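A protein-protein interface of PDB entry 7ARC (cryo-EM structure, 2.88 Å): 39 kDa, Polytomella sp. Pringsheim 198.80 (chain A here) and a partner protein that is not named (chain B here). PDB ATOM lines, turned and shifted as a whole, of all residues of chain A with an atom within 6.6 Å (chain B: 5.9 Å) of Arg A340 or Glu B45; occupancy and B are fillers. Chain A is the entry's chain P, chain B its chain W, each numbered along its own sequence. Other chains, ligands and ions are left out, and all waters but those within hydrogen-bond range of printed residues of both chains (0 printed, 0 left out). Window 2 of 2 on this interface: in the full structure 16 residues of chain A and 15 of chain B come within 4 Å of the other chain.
The side-chain carboxylate (OE2) of Glu B45 is in salt-bridge range of the guanidinium group (NE) of Arg A340 (2.8 Å). NH2 of Arg B93 lies within salt-bridge range of OE1 of Glu A337 (3.8 Å).
The guanidinium group of Arg A340 lies within hydrogen-bond range of the side-chain hydroxyl of Tyr A347.
Among the printed residues, merely in contact across the chains: Glu A337 with Ile B46 (3.2 Å), Phe A341 with Arg B93 (3.5 Å) and Tyr A347 with Lys B42 (3.4 Å).
Printed residues of chain B within 4 Å of Arg A340: Glu B45 (2.8 Å). Printed residues of chain B within 4 Å of Tyr A347: Lys B42 (3.4 Å). Printed residues of chain A within 4 Å of Lys B42: Tyr A347 (3.4 Å). Glu B45 touches one residue of chain A. The nearest residue of chain B that does not touch Arg A340 is Arg B93 (4.6 Å).
Among the printed residues, 5 pairs touch across the chains. Among the printed residues, Asp or Glu carboxylates within 4 Å of a Lys or Arg side-chain nitrogen of the other chain: Glu A337 with Arg B93 and Arg A340 with Glu B45.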
ATOM      1  N   THR A 259      15.264   0.940  11.045  1.00  0.00           N
ATOM      2  CA  THR A 259      16.380   0.398  11.812  1.00  0.00           C
ATOM      3  C   THR A 259      16.242   0.728  13.293  1.00  0.00           C
ATOM      4  O   THR A 259      16.431  -0.139  14.153  1.00  0.00           O
ATOM      5  CB  THR A 259      17.701   0.941  11.264  1.00  0.00           C
ATOM      6  OG1 THR A 259      17.842   0.558   9.890  1.00  0.00           O
ATOM      7  CG2 THR A 259      18.873   0.396  12.058  1.00  0.00           C
ATOM      8  N   LEU A 260      15.910   1.980  13.611  1.00  0.00           N
ATOM      9  CA  LEU A 260      15.685   2.374  14.995  1.00  0.00           C
ATOM     10  C   LEU A 260      14.398   1.816  15.591  1.00  0.00           C
ATOM     11  O   LEU A 260      14.228   1.900  16.813  1.00  0.00           O
ATOM     12  CB  LEU A 260      15.654   3.897  15.100  1.00  0.00           C
ATOM     13  CG  LEU A 260      17.003   4.606  15.073  1.00  0.00           C
ATOM     14  CD1 LEU A 260      16.826   6.093  15.327  1.00  0.00           C
ATOM     15  CD2 LEU A 260      17.938   3.984  16.082  1.00  0.00           C
ATOM     16  N   GLU A 332      23.747  -0.803   4.994  1.00  0.00           N
ATOM     17  CA  GLU A 332      23.917  -2.151   5.515  1.00  0.00           C
ATOM     18  C   GLU A 332      25.375  -2.366   5.893  1.00  0.00           C
ATOM     19  O   GLU A 332      26.269  -1.651   5.436  1.00  0.00           O
ATOM     20  CB  GLU A 332      23.445  -3.200   4.499  1.00  0.00           C
ATOM     21  CG  GLU A 332      24.199  -3.193   3.174  1.00  0.00           C
ATOM     22  CD  GLU A 332      25.466  -4.024   3.206  1.00  0.00           C
ATOM     23  OE1 GLU A 332      25.585  -4.896   4.092  1.00  0.00           O
ATOM     24  OE2 GLU A 332      26.343  -3.804   2.345  1.00  0.00           O
ATOM     25  N   GLY A 333      25.603  -3.370   6.739  1.00  0.00           N
ATOM     26  CA  GLY A 333      26.957  -3.745   7.101  1.00  0.00           C
ATOM     27  C   GLY A 333      27.503  -2.906   8.245  1.00  0.00           C
ATOM     28  O   GLY A 333      26.772  -2.457   9.127  1.00  0.00           O
ATOM     29  N   ILE A 336      26.290   0.848   9.062  1.00  0.00           N
ATOM     30  CA  ILE A 336      25.007   1.119   9.699  1.00  0.00           C
ATOM     31  C   ILE A 336      24.989   0.647  11.156  1.00  0.00           C
ATOM     32  O   ILE A 336      23.975   0.805  11.858  1.00  0.00           O
ATOM     33  CB  ILE A 336      23.900   0.423   8.873  1.00  0.00           C
ATOM     34  CG1 ILE A 336      22.490   0.868   9.247  1.00  0.00           C
ATOM     35  CG2 ILE A 336      23.989  -1.082   9.035  1.00  0.00           C
ATOM     36  CD1 ILE A 336      22.246   2.312   8.888  1.00  0.00           C
ATOM     37  N   GLU A 337      26.113   0.108  11.640  1.00  0.00           N
ATOM     38  CA  GLU A 337      26.211  -0.368  13.019  1.00  0.00           C
ATOM     39  C   GLU A 337      25.966   0.739  14.036  1.00  0.00           C
ATOM     40  O   GLU A 337      25.420   0.481  15.114  1.00  0.00           O
ATOM     41  CB  GLU A 337      27.575  -1.011  13.264  1.00  0.00           C
ATOM     42  CG  GLU A 337      27.810  -2.301  12.506  1.00  0.00           C
ATOM     43  CD  GLU A 337      29.181  -2.886  12.780  1.00  0.00           C
ATOM     44  OE1 GLU A 337      29.985  -2.220  13.465  1.00  0.00           O
ATOM     45  OE2 GLU A 337      29.459  -4.005  12.302  1.00  0.00           O
ATOM     46  N   GLY A 338      26.440   1.957  13.762  1.00  0.00           N
ATOM     47  CA  GLY A 338      26.331   3.001  14.771  1.00  0.00           C
ATOM     48  C   GLY A 338      24.892   3.315  15.129  1.00  0.00           C
ATOM     49  O   GLY A 338      24.534   3.385  16.308  1.00  0.00           O
ATOM     50  N   VAL A 339      24.045   3.514  14.117  1.00  0.00           N
ATOM     51  CA  VAL A 339      22.622   3.693  14.382  1.00  0.00           C
ATOM     52  C   VAL A 339      22.013   2.393  14.883  1.00  0.00           C
ATOM     53  O   VAL A 339      21.040   2.407  15.647  1.00  0.00           O
ATOM     54  CB  VAL A 339      21.885   4.220  13.138  1.00  0.00           C
ATOM     55  CG1 VAL A 339      21.935   3.209  12.060  1.00  0.00           C
ATOM     56  CG2 VAL A 339      20.436   4.528  13.468  1.00  0.00           C
ATOM     57  N   ARG A 340      22.575   1.251  14.473  1.00  0.00           N
ATOM     58  CA  ARG A 340      22.010  -0.033  14.873  1.00  0.00           C
ATOM     59  C   ARG A 340      22.124  -0.243  16.379  1.00  0.00           C
ATOM     60  O   ARG A 340      21.220  -0.807  17.006  1.00  0.00           O
ATOM     61  CB  ARG A 340      22.716  -1.169  14.139  1.00  0.00           C
ATOM     62  CG  ARG A 340      21.905  -2.442  14.091  1.00  0.00           C
ATOM     63  CD  ARG A 340      22.727  -3.704  14.190  1.00  0.00           C
ATOM     64  NE  ARG A 340      23.713  -3.670  15.264  1.00  0.00           N
ATOM     65  CZ  ARG A 340      23.540  -4.262  16.439  1.00  0.00           C
ATOM     66  NH1 ARG A 340      22.456  -4.973  16.701  1.00  0.00           N
ATOM     67  NH2 ARG A 340      24.491  -4.166  17.364  1.00  0.00           N
ATOM     68  N   PHE A 341      23.232   0.206  16.970  1.00  0.00           N
ATOM     69  CA  PHE A 341      23.455   0.023  18.404  1.00  0.00           C
ATOM     70  C   PHE A 341      22.379   0.690  19.254  1.00  0.00           C
ATOM     71  O   PHE A 341      22.071   0.198  20.346  1.00  0.00           O
ATOM     72  CB  PHE A 341      24.824   0.574  18.814  1.00  0.00           C
ATOM     73  CG  PHE A 341      25.996  -0.193  18.265  1.00  0.00           C
ATOM     74  CD1 PHE A 341      25.832  -1.451  17.719  1.00  0.00           C
ATOM     75  CD2 PHE A 341      27.274   0.340  18.325  1.00  0.00           C
ATOM     76  CE1 PHE A 341      26.916  -2.156  17.224  1.00  0.00           C
ATOM     77  CE2 PHE A 341      28.360  -0.361  17.834  1.00  0.00           C
ATOM     78  CZ  PHE A 341      28.180  -1.609  17.284  1.00  0.00           C
ATOM     79  N   ILE A 342      21.816   1.807  18.795  1.00  0.00           N
ATOM     80  CA  ILE A 342      20.785   2.515  19.548  1.00  0.00           C
ATOM     81  C   ILE A 342      19.608   1.608  19.894  1.00  0.00           C
ATOM     82  O   ILE A 342      19.399   1.279  21.067  1.00  0.00           O
ATOM     83  CB  ILE A 342      20.303   3.758  18.778  1.00  0.00           C
ATOM     84  CG1 ILE A 342      21.460   4.737  18.568  1.00  0.00           C
ATOM     85  CG2 ILE A 342      19.166   4.438  19.522  1.00  0.00           C
ATOM     86  CD1 ILE A 342      22.183   5.106  19.839  1.00  0.00           C
ATOM     87  N   ARG A 343      18.860   1.164  18.882  1.00  0.00           N
ATOM     88  CA  ARG A 343      17.727   0.262  19.070  1.00  0.00           C
ATOM     89  C   ARG A 343      17.505  -0.542  17.797  1.00  0.00           C
ATOM     90  O   ARG A 343      17.613  -0.006  16.691  1.00  0.00           O
ATOM     91  CB  ARG A 343      16.432   1.003  19.446  1.00  0.00           C
ATOM     92  CG  ARG A 343      16.434   1.640  20.829  1.00  0.00           C
ATOM     93  CD  ARG A 343      15.107   2.288  21.188  1.00  0.00           C
ATOM     94  NE  ARG A 343      14.831   3.478  20.394  1.00  0.00           N
ATOM     95  CZ  ARG A 343      13.855   3.572  19.504  1.00  0.00           C
ATOM     96  NH1 ARG A 343      13.028   2.564  19.276  1.00  0.00           N
ATOM     97  NH2 ARG A 343      13.698   4.708  18.832  1.00  0.00           N
ATOM     98  N   VAL A 344      17.198  -1.830  17.963  1.00  0.00           N
ATOM     99  CA  VAL A 344      16.782  -2.690  16.858  1.00  0.00           C
ATOM    100  C   VAL A 344      15.544  -3.497  17.219  1.00  0.00           C
ATOM    101  O   VAL A 344      15.223  -4.488  16.553  1.00  0.00           O
ATOM    102  CB  VAL A 344      17.915  -3.637  16.427  1.00  0.00           C
ATOM    103  CG1 VAL A 344      19.086  -2.851  15.926  1.00  0.00           C
ATOM    104  CG2 VAL A 344      18.332  -4.528  17.591  1.00  0.00           C
ATOM    105  N   TYR A 347      16.770  -4.841  21.208  1.00  0.00           N
ATOM    106  CA  TYR A 347      17.421  -3.987  22.187  1.00  0.00           C
ATOM    107  C   TYR A 347      16.386  -3.189  22.973  1.00  0.00           C
ATOM    108  O   TYR A 347      15.326  -2.831  22.452  1.00  0.00           O
ATOM    109  CB  TYR A 347      18.383  -3.024  21.489  1.00  0.00           C
ATOM    110  CG  TYR A 347      19.730  -3.619  21.154  1.00  0.00           C
ATOM    111  CD1 TYR A 347      19.977  -4.974  21.324  1.00  0.00           C
ATOM    112  CD2 TYR A 347      20.753  -2.825  20.654  1.00  0.00           C
ATOM    113  CE1 TYR A 347      21.206  -5.518  21.014  1.00  0.00           C
ATOM    114  CE2 TYR A 347      21.985  -3.361  20.341  1.00  0.00           C
ATOM    115  CZ  TYR A 347      22.206  -4.707  20.523  1.00  0.00           C
ATOM    116  OH  TYR A 347      23.432  -5.245  20.209  1.00  0.00           O
ATOM    117  N   LYS B  42      26.118 -11.357  18.711  1.00  0.00           N
ATOM    118  CA  LYS B  42      25.352 -10.273  18.085  1.00  0.00           C
ATOM    119  C   LYS B  42      25.822 -10.002  16.657  1.00  0.00           C
ATOM    120  O   LYS B  42      25.960  -8.854  16.231  1.00  0.00           O
ATOM    121  CB  LYS B  42      25.432  -8.996  18.925  1.00  0.00           C
ATOM    122  CG  LYS B  42      24.848  -9.117  20.321  1.00  0.00           C
ATOM    123  CD  LYS B  42      23.343  -9.273  20.280  1.00  0.00           C
ATOM    124  CE  LYS B  42      22.769  -9.394  21.679  1.00  0.00           C
ATOM    125  NZ  LYS B  42      22.906  -8.122  22.440  1.00  0.00           N
ATOM    126  N   LEU B  43      26.069 -11.075  15.909  1.00  0.00           N
ATOM    127  CA  LEU B  43      26.623 -10.986  14.567  1.00  0.00           C
ATOM    128  C   LEU B  43      25.587 -11.213  13.473  1.00  0.00           C
ATOM    129  O   LEU B  43      25.966 -11.418  12.316  1.00  0.00           O
ATOM    130  CB  LEU B  43      27.765 -11.990  14.407  1.00  0.00           C
ATOM    131  CG  LEU B  43      29.005 -11.752  15.266  1.00  0.00           C
ATOM    132  CD1 LEU B  43      29.991 -12.893  15.103  1.00  0.00           C
ATOM    133  CD2 LEU B  43      29.650 -10.427  14.922  1.00  0.00           C
ATOM    134  N   GLU B  44      24.293 -11.199  13.812  1.00  0.00           N
ATOM    135  CA  GLU B  44      23.262 -11.523  12.827  1.00  0.00           C
ATOM    136  C   GLU B  44      23.307 -10.559  11.649  1.00  0.00           C
ATOM    137  O   GLU B  44      23.334 -10.977  10.486  1.00  0.00           O
ATOM    138  CB  GLU B  44      21.876 -11.477  13.471  1.00  0.00           C
ATOM    139  CG  GLU B  44      21.602 -12.524  14.532  1.00  0.00           C
ATOM    140  CD  GLU B  44      22.127 -12.117  15.893  1.00  0.00           C
ATOM    141  OE1 GLU B  44      22.650 -10.991  16.024  1.00  0.00           O
ATOM    142  OE2 GLU B  44      21.992 -12.914  16.839  1.00  0.00           O
ATOM    143  N   GLU B  45      23.301  -9.260  11.939  1.00  0.00           N
ATOM    144  CA  GLU B  45      23.184  -8.251  10.893  1.00  0.00           C
ATOM    145  C   GLU B  45      24.458  -8.149  10.062  1.00  0.00           C
ATOM    146  O   GLU B  45      24.398  -7.938   8.845  1.00  0.00           O
ATOM    147  CB  GLU B  45      22.844  -6.900  11.520  1.00  0.00           C
ATOM    148  CG  GLU B  45      23.982  -6.312  12.341  1.00  0.00           C
ATOM    149  CD  GLU B  45      24.026  -6.840  13.764  1.00  0.00           C
ATOM    150  OE1 GLU B  45      23.375  -7.868  14.047  1.00  0.00           O
ATOM    151  OE2 GLU B  45      24.736  -6.239  14.595  1.00  0.00           O
ATOM    152  N   ILE B  46      25.621  -8.294  10.700  1.00  0.00           N
ATOM    153  CA  ILE B  46      26.887  -8.105  10.002  1.00  0.00           C
ATOM    154  C   ILE B  46      27.149  -9.245   9.027  1.00  0.00           C
ATOM    155  O   ILE B  46      27.542  -9.016   7.877  1.00  0.00           O
ATOM    156  CB  ILE B  46      28.029  -7.960  11.023  1.00  0.00           C
ATOM    157  CG1 ILE B  46      27.619  -6.971  12.115  1.00  0.00           C
ATOM    158  CG2 ILE B  46      29.307  -7.510  10.336  1.00  0.00           C
ATOM    159  CD1 ILE B  46      28.554  -6.928  13.287  1.00  0.00           C
ATOM    160  N   THR B  47      26.937 -10.485   9.460  1.00  0.00           N
ATOM    161  CA  THR B  47      27.311 -11.623   8.637  1.00  0.00           C
ATOM    162  C   THR B  47      26.212 -12.673   8.662  1.00  0.00           C
ATOM    163  O   THR B  47      25.419 -12.761   9.603  1.00  0.00           O
ATOM    164  CB  THR B  47      28.643 -12.233   9.098  1.00  0.00           C
ATOM    165  OG1 THR B  47      29.087 -13.202   8.140  1.00  0.00           O
ATOM    166  CG2 THR B  47      28.490 -12.897  10.455  1.00  0.00           C
ATOM    167  N   ARG B  93      33.135  -9.702  20.463  1.00  0.00           N
ATOM    168  CA  ARG B  93      32.541  -9.410  19.161  1.00  0.00           C
ATOM    169  C   ARG B  93      33.550  -8.759  18.230  1.00  0.00           C
ATOM    170  O   ARG B  93      33.647  -9.123  17.051  1.00  0.00           O
ATOM    171  CB  ARG B  93      31.326  -8.498  19.331  1.00  0.00           C
ATOM    172  CG  ARG B  93      30.657  -8.119  18.025  1.00  0.00           C
ATOM    173  CD  ARG B  93      29.239  -7.616  18.243  1.00  0.00           C
ATOM    174  NE  ARG B  93      28.795  -6.733  17.170  1.00  0.00           N
ATOM    175  CZ  ARG B  93      29.265  -5.513  16.953  1.00  0.00           C
ATOM    176  NH1 ARG B  93      30.191  -4.977  17.732  1.00  0.00           N
ATOM    177  NH2 ARG B  93      28.797  -4.811  15.926  1.00  0.00           N
